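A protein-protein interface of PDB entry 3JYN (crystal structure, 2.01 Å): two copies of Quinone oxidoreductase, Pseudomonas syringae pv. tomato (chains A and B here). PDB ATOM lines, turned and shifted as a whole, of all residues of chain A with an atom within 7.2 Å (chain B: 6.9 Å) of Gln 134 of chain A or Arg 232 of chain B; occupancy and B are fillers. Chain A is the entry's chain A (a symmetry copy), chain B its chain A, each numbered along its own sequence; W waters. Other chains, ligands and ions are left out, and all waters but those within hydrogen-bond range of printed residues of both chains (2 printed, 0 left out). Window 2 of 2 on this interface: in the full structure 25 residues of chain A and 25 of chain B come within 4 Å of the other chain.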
ATOM      1  N   LEU A 126      24.071 -20.248 -15.047  1.00  0.00           N
ATOM      2  CA  LEU A 126      23.017 -19.247 -14.892  1.00  0.00           C
ATOM      3  C   LEU A 126      22.407 -19.361 -13.497  1.00  0.00           C
ATOM      4  O   LEU A 126      21.987 -18.365 -12.906  1.00  0.00           O
ATOM      5  CB  LEU A 126      21.923 -19.446 -15.951  1.00  0.00           C
ATOM      6  CG  LEU A 126      22.293 -19.046 -17.384  1.00  0.00           C
ATOM      7  CD1 LEU A 126      21.168 -19.423 -18.340  1.00  0.00           C
ATOM      8  CD2 LEU A 126      22.555 -17.543 -17.437  1.00  0.00           C
ATOM      9  N   VAL A 128      24.018 -20.473 -10.696  1.00  0.00           N
ATOM     10  CA  VAL A 128      24.965 -19.921  -9.730  1.00  0.00           C
ATOM     11  C   VAL A 128      24.901 -18.400  -9.803  1.00  0.00           C
ATOM     12  O   VAL A 128      25.005 -17.713  -8.791  1.00  0.00           O
ATOM     13  CB  VAL A 128      26.419 -20.360 -10.025  1.00  0.00           C
ATOM     14  CG1 VAL A 128      27.392 -19.565  -9.155  1.00  0.00           C
ATOM     15  CG2 VAL A 128      26.582 -21.851  -9.749  1.00  0.00           C
ATOM     16  N   GLN A 129      24.738 -17.873 -11.011  1.00  0.00           N
ATOM     17  CA  GLN A 129      24.655 -16.430 -11.176  1.00  0.00           C
ATOM     18  C   GLN A 129      23.496 -15.849 -10.369  1.00  0.00           C
ATOM     19  O   GLN A 129      23.694 -14.922  -9.583  1.00  0.00           O
ATOM     20  CB  GLN A 129      24.492 -16.070 -12.656  1.00  0.00           C
ATOM     21  CG  GLN A 129      24.687 -14.588 -12.999  1.00  0.00           C
ATOM     22  CD  GLN A 129      23.528 -13.716 -12.554  1.00  0.00           C
ATOM     23  OE1 GLN A 129      22.386 -14.171 -12.493  1.00  0.00           O
ATOM     24  NE2 GLN A 129      23.811 -12.451 -12.262  1.00  0.00           N
ATOM     25  N   TYR A 130      22.291 -16.393 -10.532  1.00  0.00           N
ATOM     26  CA  TYR A 130      21.163 -15.836  -9.800  1.00  0.00           C
ATOM     27  C   TYR A 130      21.231 -16.171  -8.312  1.00  0.00           C
ATOM     28  O   TYR A 130      20.806 -15.375  -7.480  1.00  0.00           O
ATOM     29  CB  TYR A 130      19.817 -16.262 -10.437  1.00  0.00           C
ATOM     30  CG  TYR A 130      19.216 -17.587  -9.997  1.00  0.00           C
ATOM     31  CD1 TYR A 130      18.738 -17.767  -8.695  1.00  0.00           C
ATOM     32  CD2 TYR A 130      19.075 -18.644 -10.898  1.00  0.00           C
ATOM     33  CE1 TYR A 130      18.131 -18.962  -8.302  1.00  0.00           C
ATOM     34  CE2 TYR A 130      18.467 -19.847 -10.516  1.00  0.00           C
ATOM     35  CZ  TYR A 130      17.999 -19.996  -9.215  1.00  0.00           C
ATOM     36  OH  TYR A 130      17.403 -21.171  -8.823  1.00  0.00           O
ATOM     37  N   LEU A 131      21.788 -17.327  -7.966  1.00  0.00           N
ATOM     38  CA  LEU A 131      21.907 -17.688  -6.563  1.00  0.00           C
ATOM     39  C   LEU A 131      22.839 -16.741  -5.808  1.00  0.00           C
ATOM     40  O   LEU A 131      22.508 -16.275  -4.716  1.00  0.00           O
ATOM     41  CB  LEU A 131      22.432 -19.117  -6.412  1.00  0.00           C
ATOM     42  CG  LEU A 131      21.480 -20.259  -6.749  1.00  0.00           C
ATOM     43  CD1 LEU A 131      22.216 -21.579  -6.588  1.00  0.00           C
ATOM     44  CD2 LEU A 131      20.252 -20.207  -5.846  1.00  0.00           C
ATOM     45  N   LEU A 132      23.997 -16.442  -6.391  1.00  0.00           N
ATOM     46  CA  LEU A 132      24.974 -15.580  -5.724  1.00  0.00           C
ATOM     47  C   LEU A 132      24.865 -14.087  -5.998  1.00  0.00           C
ATOM     48  O   LEU A 132      25.452 -13.286  -5.267  1.00  0.00           O
ATOM     49  CB  LEU A 132      26.400 -16.023  -6.075  1.00  0.00           C
ATOM     50  CG  LEU A 132      26.776 -17.491  -5.852  1.00  0.00           C
ATOM     51  CD1 LEU A 132      28.255 -17.672  -6.178  1.00  0.00           C
ATOM     52  CD2 LEU A 132      26.485 -17.909  -4.422  1.00  0.00           C
ATOM     53  N   ARG A 133      24.119 -13.709  -7.034  1.00  0.00           N
ATOM     54  CA  ARG A 133      23.988 -12.294  -7.391  1.00  0.00           C
ATOM     55  C   ARG A 133      22.589 -11.709  -7.199  1.00  0.00           C
ATOM     56  O   ARG A 133      22.445 -10.510  -6.971  1.00  0.00           O
ATOM     57  CB  ARG A 133      24.395 -12.078  -8.856  1.00  0.00           C
ATOM     58  CG  ARG A 133      25.769 -12.619  -9.256  1.00  0.00           C
ATOM     59  CD  ARG A 133      26.873 -11.734  -8.722  1.00  0.00           C
ATOM     60  NE  ARG A 133      26.836 -11.717  -7.277  1.00  0.00           N
ATOM     61  CZ  ARG A 133      27.272 -10.721  -6.521  1.00  0.00           C
ATOM     62  NH1 ARG A 133      27.797  -9.631  -7.069  1.00  0.00           N
ATOM     63  NH2 ARG A 133      27.170 -10.821  -5.209  1.00  0.00           N
ATOM     64  N   GLN A 134      21.562 -12.546  -7.288  1.00  0.00           N
ATOM     65  CA  GLN A 134      20.188 -12.058  -7.180  1.00  0.00           C
ATOM     66  C   GLN A 134      19.376 -12.545  -5.986  1.00  0.00           C
ATOM     67  O   GLN A 134      18.758 -11.747  -5.296  1.00  0.00           O
ATOM     68  CB  GLN A 134      19.423 -12.402  -8.458  1.00  0.00           C
ATOM     69  CG  GLN A 134      20.092 -11.946  -9.735  1.00  0.00           C
ATOM     70  CD  GLN A 134      19.264 -12.291 -10.954  1.00  0.00           C
ATOM     71  OE1 GLN A 134      18.138 -11.821 -11.107  1.00  0.00           O
ATOM     72  NE2 GLN A 134      19.815 -13.123 -11.826  1.00  0.00           N
ATOM     73  N   THR A 135      19.390 -13.851  -5.747  1.00  0.00           N
ATOM     74  CA  THR A 135      18.691 -14.418  -4.600  1.00  0.00           C
ATOM     75  C   THR A 135      19.229 -13.815  -3.306  1.00  0.00           C
ATOM     76  O   THR A 135      18.468 -13.473  -2.401  1.00  0.00           O
ATOM     77  CB  THR A 135      18.841 -15.949  -4.545  1.00  0.00           C
ATOM     78  OG1 THR A 135      18.459 -16.514  -5.803  1.00  0.00           O
ATOM     79  CG2 THR A 135      17.966 -16.531  -3.446  1.00  0.00           C
ATOM     80  N   TYR A 136      20.550 -13.686  -3.233  1.00  0.00           N
ATOM     81  CA  TYR A 136      21.215 -13.089  -2.082  1.00  0.00           C
ATOM     82  C   TYR A 136      22.560 -12.522  -2.517  1.00  0.00           C
ATOM     83  O   TYR A 136      23.508 -13.269  -2.756  1.00  0.00           O
ATOM     84  CB  TYR A 136      21.410 -14.126  -0.975  1.00  0.00           C
ATOM     85  CG  TYR A 136      22.125 -13.592   0.246  1.00  0.00           C
ATOM     86  CD1 TYR A 136      23.510 -13.477   0.269  1.00  0.00           C
ATOM     87  CD2 TYR A 136      21.418 -13.201   1.374  1.00  0.00           C
ATOM     88  CE1 TYR A 136      24.167 -12.990   1.382  1.00  0.00           C
ATOM     89  CE2 TYR A 136      22.066 -12.712   2.492  1.00  0.00           C
ATOM     90  CZ  TYR A 136      23.440 -12.608   2.491  1.00  0.00           C
ATOM     91  OH  TYR A 136      24.092 -12.121   3.600  1.00  0.00           O
ATOM     92  N   GLN A 137      22.636 -11.201  -2.631  1.00  0.00           N
ATOM     93  CA  GLN A 137      23.837 -10.552  -3.156  1.00  0.00           C
ATOM     94  C   GLN A 137      25.034 -10.780  -2.252  1.00  0.00           C
ATOM     95  O   GLN A 137      25.326  -9.962  -1.385  1.00  0.00           O
ATOM     96  CB  GLN A 137      23.618  -9.047  -3.292  1.00  0.00           C
ATOM     97  CG  GLN A 137      22.750  -8.640  -4.457  1.00  0.00           C
ATOM     98  CD  GLN A 137      22.602  -7.137  -4.551  1.00  0.00           C
ATOM     99  OE1 GLN A 137      23.593  -6.402  -4.565  1.00  0.00           O
ATOM    100  NE2 GLN A 137      21.360  -6.669  -4.618  1.00  0.00           N
ATOM    101  N   VAL A 138      25.729 -11.890  -2.455  1.00  0.00           N
ATOM    102  CA  VAL A 138      26.893 -12.200  -1.641  1.00  0.00           C
ATOM    103  C   VAL A 138      27.952 -11.109  -1.786  1.00  0.00           C
ATOM    104  O   VAL A 138      28.265 -10.667  -2.895  1.00  0.00           O
ATOM    105  CB  VAL A 138      27.478 -13.573  -2.035  1.00  0.00           C
ATOM    106  CG1 VAL A 138      26.402 -14.648  -1.885  1.00  0.00           C
ATOM    107  CG2 VAL A 138      27.969 -13.544  -3.461  1.00  0.00           C
ATOM    108  N   TYR A 214      22.962 -22.085   0.944  1.00  0.00           N
ATOM    109  CA  TYR A 214      22.450 -22.554  -0.340  1.00  0.00           C
ATOM    110  C   TYR A 214      22.310 -24.068  -0.238  1.00  0.00           C
ATOM    111  O   TYR A 214      23.290 -24.776   0.012  1.00  0.00           O
ATOM    112  CB  TYR A 214      23.419 -22.175  -1.457  1.00  0.00           C
ATOM    113  CG  TYR A 214      23.498 -20.687  -1.688  1.00  0.00           C
ATOM    114  CD1 TYR A 214      22.543 -20.029  -2.465  1.00  0.00           C
ATOM    115  CD2 TYR A 214      24.511 -19.927  -1.107  1.00  0.00           C
ATOM    116  CE1 TYR A 214      22.602 -18.642  -2.657  1.00  0.00           C
ATOM    117  CE2 TYR A 214      24.575 -18.551  -1.292  1.00  0.00           C
ATOM    118  CZ  TYR A 214      23.622 -17.917  -2.065  1.00  0.00           C
ATOM    119  OH  TYR A 214      23.700 -16.555  -2.250  1.00  0.00           O
ATOM    120  N   THR A 262      13.495 -19.446   0.785  1.00  0.00           N
ATOM    121  CA  THR A 262      12.946 -19.242  -0.546  1.00  0.00           C
ATOM    122  C   THR A 262      13.254 -20.488  -1.349  1.00  0.00           C
ATOM    123  O   THR A 262      14.211 -21.197  -1.054  1.00  0.00           O
ATOM    124  CB  THR A 262      13.562 -18.010  -1.255  1.00  0.00           C
ATOM    125  OG1 THR A 262      12.942 -17.836  -2.538  1.00  0.00           O
ATOM    126  CG2 THR A 262      15.067 -18.186  -1.446  1.00  0.00           C
ATOM    127  N   PRO A 264      13.729 -20.899  -5.108  1.00  0.00           N
ATOM    128  CA  PRO A 264      13.845 -20.283  -6.427  1.00  0.00           C
ATOM    129  C   PRO A 264      13.953 -21.278  -7.574  1.00  0.00           C
ATOM    130  O   PRO A 264      14.275 -22.452  -7.382  1.00  0.00           O
ATOM    131  CB  PRO A 264      15.096 -19.433  -6.281  1.00  0.00           C
ATOM    132  CG  PRO A 264      15.978 -20.334  -5.461  1.00  0.00           C
ATOM    133  CD  PRO A 264      15.034 -20.911  -4.415  1.00  0.00           C
ATOM    134  N   SER A 268      12.275 -18.416 -13.075  1.00  0.00           N
ATOM    135  CA  SER A 268      11.801 -17.172 -12.490  1.00  0.00           C
ATOM    136  C   SER A 268      12.794 -16.019 -12.595  1.00  0.00           C
ATOM    137  O   SER A 268      12.390 -14.857 -12.651  1.00  0.00           O
ATOM    138  CB  SER A 268      11.418 -17.392 -11.025  1.00  0.00           C
ATOM    139  OG  SER A 268      11.003 -16.174 -10.443  1.00  0.00           O
ATOM    140  N   TYR A 269      14.087 -16.332 -12.623  1.00  0.00           N
ATOM    141  CA  TYR A 269      15.115 -15.305 -12.727  1.00  0.00           C
ATOM    142  C   TYR A 269      15.466 -15.000 -14.178  1.00  0.00           C
ATOM    143  O   TYR A 269      15.712 -13.849 -14.543  1.00  0.00           O
ATOM    144  CB  TYR A 269      16.357 -15.726 -11.936  1.00  0.00           C
ATOM    145  CG  TYR A 269      16.136 -15.631 -10.443  1.00  0.00           C
ATOM    146  CD1 TYR A 269      15.308 -16.536  -9.779  1.00  0.00           C
ATOM    147  CD2 TYR A 269      16.712 -14.599  -9.702  1.00  0.00           C
ATOM    148  CE1 TYR A 269      15.061 -16.413  -8.409  1.00  0.00           C
ATOM    149  CE2 TYR A 269      16.472 -14.468  -8.338  1.00  0.00           C
ATOM    150  CZ  TYR A 269      15.647 -15.375  -7.698  1.00  0.00           C
ATOM    151  OH  TYR A 269      15.414 -15.241  -6.345  1.00  0.00           O
ATOM    152  N   ALA A 270      15.510 -16.041 -15.001  1.00  0.00           N
ATOM    153  CA  ALA A 270      15.760 -15.874 -16.425  1.00  0.00           C
ATOM    154  C   ALA A 270      14.427 -15.958 -17.148  1.00  0.00           C
ATOM    155  O   ALA A 270      14.262 -16.736 -18.088  1.00  0.00           O
ATOM    156  CB  ALA A 270      16.710 -16.943 -16.928  1.00  0.00           C
ATOM    157  N   ASN A 271      13.471 -15.156 -16.691  1.00  0.00           N
ATOM    158  CA  ASN A 271      12.100 -15.243 -17.187  1.00  0.00           C
ATOM    159  C   ASN A 271      11.874 -14.376 -18.410  1.00  0.00           C
ATOM    160  O   ASN A 271      10.739 -14.192 -18.829  1.00  0.00           O
ATOM    161  CB  ASN A 271      11.115 -14.846 -16.081  1.00  0.00           C
ATOM    162  CG  ASN A 271      11.084 -13.342 -15.829  1.00  0.00           C
ATOM    163  OD1 ASN A 271      12.104 -12.720 -15.512  1.00  0.00           O
ATOM    164  ND2 ASN A 271       9.902 -12.751 -15.976  1.00  0.00           N
ATOM    165  N   ASN A 275      16.452 -10.912 -19.476  1.00  0.00           N
ATOM    166  CA  ASN A 275      17.005 -11.026 -18.138  1.00  0.00           C
ATOM    167  C   ASN A 275      17.941 -12.216 -18.205  1.00  0.00           C
ATOM    168  O   ASN A 275      18.845 -12.380 -17.384  1.00  0.00           O
ATOM    169  CB  ASN A 275      15.901 -11.270 -17.111  1.00  0.00           C
ATOM    170  CG  ASN A 275      15.238  -9.986 -16.652  1.00  0.00           C
ATOM    171  OD1 ASN A 275      14.040  -9.955 -16.373  1.00  0.00           O
ATOM    172  ND2 ASN A 275      16.020  -8.915 -16.570  1.00  0.00           N
ATOM    173  N   THR A 278      21.236 -10.574 -19.908  1.00  0.00           N
ATOM    174  CA  THR A 278      22.057  -9.916 -18.907  1.00  0.00           C
ATOM    175  C   THR A 278      22.768 -10.944 -18.024  1.00  0.00           C
ATOM    176  O   THR A 278      23.948 -10.791 -17.706  1.00  0.00           O
ATOM    177  CB  THR A 278      21.204  -8.935 -18.046  1.00  0.00           C
ATOM    178  OG1 THR A 278      21.992  -8.440 -16.960  1.00  0.00           O
ATOM    179  CG2 THR A 278      19.972  -9.611 -17.507  1.00  0.00           C
ATOM    180  N   MET A 279      22.055 -11.999 -17.643  1.00  0.00           N
ATOM    181  CA  MET A 279      22.639 -13.048 -16.814  1.00  0.00           C
ATOM    182  C   MET A 279      23.703 -13.824 -17.588  1.00  0.00           C
ATOM    183  O   MET A 279      24.777 -14.118 -17.061  1.00  0.00           O
ATOM    184  CB  MET A 279      21.550 -14.001 -16.336  1.00  0.00           C
ATOM    185  CG  MET A 279      20.647 -13.403 -15.271  1.00  0.00           C
ATOM    186  SD  MET A 279      19.215 -14.429 -14.949  1.00  0.00           S
ATOM    187  CE  MET A 279      20.004 -15.922 -14.282  1.00  0.00           C
ATOM    188  N   GLU A 282      27.010 -11.990 -18.016  1.00  0.00           N
ATOM    189  CA  GLU A 282      27.868 -12.061 -16.843  1.00  0.00           C
ATOM    190  C   GLU A 282      28.555 -13.422 -16.753  1.00  0.00           C
ATOM    191  O   GLU A 282      29.741 -13.510 -16.437  1.00  0.00           O
ATOM    192  CB  GLU A 282      27.064 -11.807 -15.565  1.00  0.00           C
ATOM    193  CG  GLU A 282      27.931 -11.310 -14.415  1.00  0.00           C
ATOM    194  CD  GLU A 282      27.149 -11.047 -13.145  1.00  0.00           C
ATOM    195  OE1 GLU A 282      26.035 -10.487 -13.230  1.00  0.00           O
ATOM    196  OE2 GLU A 282      27.662 -11.386 -12.057  1.00  0.00           O
ATOM    197  N   PRO B 211       5.126  -6.281  -3.404  1.00  0.00           N
ATOM    198  CA  PRO B 211       6.496  -6.711  -3.111  1.00  0.00           C
ATOM    199  C   PRO B 211       6.583  -7.399  -1.752  1.00  0.00           C
ATOM    200  O   PRO B 211       7.458  -8.232  -1.523  1.00  0.00           O
ATOM    201  CB  PRO B 211       7.295  -5.408  -3.174  1.00  0.00           C
ATOM    202  CG  PRO B 211       6.270  -4.347  -2.842  1.00  0.00           C
ATOM    203  CD  PRO B 211       5.050  -4.820  -3.577  1.00  0.00           C
ATOM    204  N   VAL B 229       1.413 -11.861  -3.424  1.00  0.00           N
ATOM    205  CA  VAL B 229       2.811 -11.435  -3.457  1.00  0.00           C
ATOM    206  C   VAL B 229       3.342 -11.387  -4.885  1.00  0.00           C
ATOM    207  O   VAL B 229       2.988 -12.221  -5.719  1.00  0.00           O
ATOM    208  CB  VAL B 229       3.705 -12.367  -2.617  1.00  0.00           C
ATOM    209  CG1 VAL B 229       4.030 -13.633  -3.395  1.00  0.00           C
ATOM    210  CG2 VAL B 229       4.978 -11.646  -2.202  1.00  0.00           C
ATOM    211  N   ALA B 230       4.194 -10.405  -5.160  1.00  0.00           N
ATOM    212  CA  ALA B 230       4.829 -10.281  -6.467  1.00  0.00           C
ATOM    213  C   ALA B 230       5.922 -11.336  -6.616  1.00  0.00           C
ATOM    214  O   ALA B 230       6.420 -11.876  -5.623  1.00  0.00           O
ATOM    215  CB  ALA B 230       5.429  -8.882  -6.618  1.00  0.00           C
ATOM    216  N   PRO B 231       6.306 -11.654  -7.862  1.00  0.00           N
ATOM    217  CA  PRO B 231       7.352 -12.657  -8.072  1.00  0.00           C
ATOM    218  C   PRO B 231       8.592 -12.300  -7.252  1.00  0.00           C
ATOM    219  O   PRO B 231       8.969 -11.133  -7.174  1.00  0.00           O
ATOM    220  CB  PRO B 231       7.602 -12.575  -9.573  1.00  0.00           C
ATOM    221  CG  PRO B 231       6.244 -12.232 -10.112  1.00  0.00           C
ATOM    222  CD  PRO B 231       5.782 -11.161  -9.150  1.00  0.00           C
ATOM    223  N   ARG B 232       9.217 -13.299  -6.635  1.00  0.00           N
ATOM    224  CA  ARG B 232      10.411 -13.050  -5.826  1.00  0.00           C
ATOM    225  C   ARG B 232      10.119 -12.065  -4.689  1.00  0.00           C
ATOM    226  O   ARG B 232      11.030 -11.427  -4.150  1.00  0.00           O
ATOM    227  CB  ARG B 232      11.542 -12.494  -6.702  1.00  0.00           C
ATOM    228  CG  ARG B 232      12.087 -13.471  -7.739  1.00  0.00           C
ATOM    229  CD  ARG B 232      13.090 -12.786  -8.674  1.00  0.00           C
ATOM    230  NE  ARG B 232      14.161 -12.121  -7.931  1.00  0.00           N
ATOM    231  CZ  ARG B 232      15.143 -11.408  -8.482  1.00  0.00           C
ATOM    232  NH1 ARG B 232      15.206 -11.257  -9.799  1.00  0.00           N
ATOM    233  NH2 ARG B 232      16.063 -10.843  -7.711  1.00  0.00           N
ATOM    234  N   GLY B 233       8.846 -11.948  -4.328  1.00  0.00           N
ATOM    235  CA  GLY B 233       8.454 -11.047  -3.260  1.00  0.00           C
ATOM    236  C   GLY B 233       8.487 -11.760  -1.923  1.00  0.00           C
ATOM    237  O   GLY B 233       8.831 -12.935  -1.862  1.00  0.00           O
ATOM    238  N   LEU B 234       8.111 -11.067  -0.853  1.00  0.00           N
ATOM    239  CA  LEU B 234       8.152 -11.672   0.478  1.00  0.00           C
ATOM    240  C   LEU B 234       6.817 -11.748   1.200  1.00  0.00           C
ATOM    241  O   LEU B 234       6.056 -10.784   1.209  1.00  0.00           O
ATOM    242  CB  LEU B 234       9.144 -10.898   1.359  1.00  0.00           C
ATOM    243  CG  LEU B 234       9.199 -11.205   2.862  1.00  0.00           C
ATOM    244  CD1 LEU B 234       9.939 -12.516   3.117  1.00  0.00           C
ATOM    245  CD2 LEU B 234       9.908 -10.053   3.574  1.00  0.00           C
ATOM    246  N   LEU B 253       6.578 -22.372  -2.949  1.00  0.00           N
ATOM    247  CA  LEU B 253       7.228 -21.068  -3.052  1.00  0.00           C
ATOM    248  C   LEU B 253       7.702 -20.858  -4.485  1.00  0.00           C
ATOM    249  O   LEU B 253       7.671 -19.745  -5.005  1.00  0.00           O
ATOM    250  CB  LEU B 253       8.425 -20.980  -2.098  1.00  0.00           C
ATOM    251  CG  LEU B 253       8.148 -21.166  -0.602  1.00  0.00           C
ATOM    252  CD1 LEU B 253       9.463 -21.036   0.164  1.00  0.00           C
ATOM    253  CD2 LEU B 253       7.150 -20.126  -0.119  1.00  0.00           C
ATOM    254  N   LYS B 256       4.668 -20.305  -6.817  1.00  0.00           N
ATOM    255  CA  LYS B 256       4.158 -18.938  -6.766  1.00  0.00           C
ATOM    256  C   LYS B 256       5.167 -17.922  -7.299  1.00  0.00           C
ATOM    257  O   LYS B 256       5.099 -16.733  -6.980  1.00  0.00           O
ATOM    258  CB  LYS B 256       3.756 -18.576  -5.336  1.00  0.00           C
ATOM    259  CG  LYS B 256       2.687 -19.484  -4.755  1.00  0.00           C
ATOM    260  CD  LYS B 256       1.404 -19.459  -5.581  1.00  0.00           C
ATOM    261  CE  LYS B 256       0.370 -20.428  -5.014  1.00  0.00           C
ATOM    262  NZ  LYS B 256      -0.929 -20.377  -5.752  1.00  0.00           N
ATOM    263  N   ASP B 257       6.101 -18.412  -8.110  1.00  0.00           N
ATOM    264  CA  ASP B 257       7.133 -17.602  -8.757  1.00  0.00           C
ATOM    265  C   ASP B 257       8.323 -17.207  -7.883  1.00  0.00           C
ATOM    266  O   ASP B 257       8.679 -16.032  -7.781  1.00  0.00           O
ATOM    267  CB  ASP B 257       6.500 -16.359  -9.382  1.00  0.00           C
ATOM    268  CG  ASP B 257       7.166 -15.958 -10.690  1.00  0.00           C
ATOM    269  OD1 ASP B 257       6.574 -15.138 -11.424  1.00  0.00           O
ATOM    270  OD2 ASP B 257       8.279 -16.456 -10.988  1.00  0.00           O
ATOM    271  N   SER B 258       8.933 -18.207  -7.256  1.00  0.00           N
ATOM    272  CA  SER B 258      10.117 -18.017  -6.423  1.00  0.00           C
ATOM    273  C   SER B 258      10.021 -16.940  -5.347  1.00  0.00           C
ATOM    274  O   SER B 258      10.854 -16.040  -5.281  1.00  0.00           O
ATOM    275  CB  SER B 258      11.318 -17.728  -7.321  1.00  0.00           C
ATOM    276  OG  SER B 258      11.518 -18.787  -8.238  1.00  0.00           O
ATOM    277  N   VAL B 259       9.025 -17.050  -4.480  1.00  0.00           N
ATOM    278  CA  VAL B 259       8.861 -16.069  -3.423  1.00  0.00           C
ATOM    279  C   VAL B 259       9.630 -16.460  -2.165  1.00  0.00           C
ATOM    280  O   VAL B 259      10.213 -17.551  -2.079  1.00  0.00           O
ATOM    281  CB  VAL B 259       7.362 -15.865  -3.080  1.00  0.00           C
ATOM    282  CG1 VAL B 259       6.637 -15.258  -4.281  1.00  0.00           C
ATOM    283  CG2 VAL B 259       6.722 -17.191  -2.696  1.00  0.00           C
ATOM    284  N   TYR B 260       9.661 -15.538  -1.209  1.00  0.00           N
ATOM    285  CA  TYR B 260      10.332 -15.755   0.066  1.00  0.00           C
ATOM    286  C   TYR B 260       9.288 -15.739   1.179  1.00  0.00           C
ATOM    287  O   TYR B 260       8.234 -15.117   1.044  1.00  0.00           O
ATOM    288  CB  TYR B 260      11.325 -14.630   0.376  1.00  0.00           C
ATOM    289  CG  TYR B 260      12.474 -14.443  -0.588  1.00  0.00           C
ATOM    290  CD1 TYR B 260      12.249 -14.061  -1.914  1.00  0.00           C
ATOM    291  CD2 TYR B 260      13.794 -14.571  -0.153  1.00  0.00           C
ATOM    292  CE1 TYR B 260      13.308 -13.801  -2.774  1.00  0.00           C
ATOM    293  CE2 TYR B 260      14.866 -14.313  -1.010  1.00  0.00           C
ATOM    294  CZ  TYR B 260      14.613 -13.924  -2.318  1.00  0.00           C
ATOM    295  OH  TYR B 260      15.659 -13.633  -3.162  1.00  0.00           O
HETATM  296  O   HOH W   1      15.107 -12.196  -5.504  1.00  0.00           O
HETATM  297  O   HOH W   2      13.567 -16.572  -4.939  1.00  0.00           O
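Gln 134 of chain A touches one residue of chain B. Tyr 136 of chain A touches none of the printed residues of chain B. Printed residues of chain B within 4 Å of Thr 262 of chain A: Leu 253 (3.98 Å), Ser 258 (3.9 Å), Val 259 (2.8 Å) and Tyr 260 (3.6 Å). Arg 232 of chain B touches three residues of chain A. Of the printed residues of chain A, Asp 257 of chain B touches Ser 268 (2.8 Å). The nearest residue of chain B that does not touch Gln 134 of chain A is Tyr 260 of chain B (4.2 Å). The nearest residue of chain A that does not touch Arg 232 of chain B is Thr 135 of chain A (4.9 Å).
No position is printed for both chains.
Of the 23 printed residues of chain A, 6 touch a printed residue of chain B. Printed residues of chain A that touch a printed residue of chain B: Gln 134, Thr 135, Thr 262, Pro 264, Ser 268 and Tyr 269. Hydrophobic or aromatic side chains of chain A that line the printed part of chain B: Tyr 269. Of the 13 printed residues of chain B, 6 touch a printed residue of chain A. Printed residues of chain B that touch a printed residue of chain A: Arg 232, Leu 253, Asp 257, Ser 258, Val 259 and Tyr 260. Hydrophobic or aromatic side chains of chain B within 4 Å of the printed part of chain A: Leu 253 and Tyr 260. Among the printed residues, no Asp or Glu carboxylate lies within 4 Å of a Lys or Arg side-chain nitrogen of the other chain.
Water W1 lies within hydrogen-bond range of NE of Arg 232 of chain B (2.6 Å), OH of Tyr 260 of chain B (2.8 Å) and OH of Tyr 269 of chain A (3.2 Å). Water W2 lies within hydrogen-bond range of OH of Tyr 269 of chain A (2.7 Å), OG1 of Thr 262 of chain A (2.8 Å) and O of Ser 258 of chain B (2.8 Å).
The backbone carbonyl oxygen (O) of Asp 257 of chain B sits at hydrogen-bond distance from the backbone NH (N) of Arg 232 of chain B, at 3.0 Å. The backbone NH (N) of Tyr 260 of chain B sits at hydrogen-bond distance from the backbone carbonyl oxygen (O) of Gly 233 of chain B (2.8 Å). OE1 of Gln 129 of chain A is in hydrogen-bond range of NE2 of Gln 134 of chain A (2.9 Å). The backbone carbonyl oxygen of Tyr 130 of chain A lies within hydrogen-bond range of the backbone NH of Thr 135 of chain A (2.7 Å). The side-chain amide nitrogen (NE2) of Gln 134 of chain A lies within hydrogen-bond range of the side-chain sulfur (SD) of Met 279 of chain A (3.4 Å). The side-chain hydroxyl (OG1) of Thr 135 of chain A lies within hydrogen-bond range of the side-chain hydroxyl (OH) of Tyr 269 of chain A (3.3 Å).
Thr 262 of chain A touches Leu 253 of chain B. Thr 262 of chain A touches Ser 258 of chain B (OG1 to O, 3.9 Å). Thr 262 of chain A touches Tyr 260 of chain B (CB to CD2, 3.6 Å). Ser 258 of chain B touches Pro 264 of chain A. Ser 268 of chain A touches Arg 232 of chain B. Tyr 269 of chain A touches Arg 232 of chain B (CE2 to NE, 3.3 Å). Tyr 260 of chain B touches Tyr 269 of chain A (OH to OH, 3.6 Å).
OE1 of Gln 134 of chain A lies within hydrogen-bond range of NH1 of Arg 232 of chain B (3.3 Å). OD2 of Asp 257 of chain B is in hydrogen-bond range of OG of Ser 268 of chain A (2.8 Å). OG of Ser 258 of chain B lies close to OG of Ser 268 of chain A (3.5 Å). The backbone carbonyl oxygen of Val 259 of chain B lies within hydrogen-bond range of the side-chain hydroxyl of Thr 262 of chain A, at 2.8 Å. The side-chain hydroxyl of Tyr 260 of chain B lies within hydrogen-bond range of the backbone carbonyl oxygen of Thr 135 of chain A (2.9 Å).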
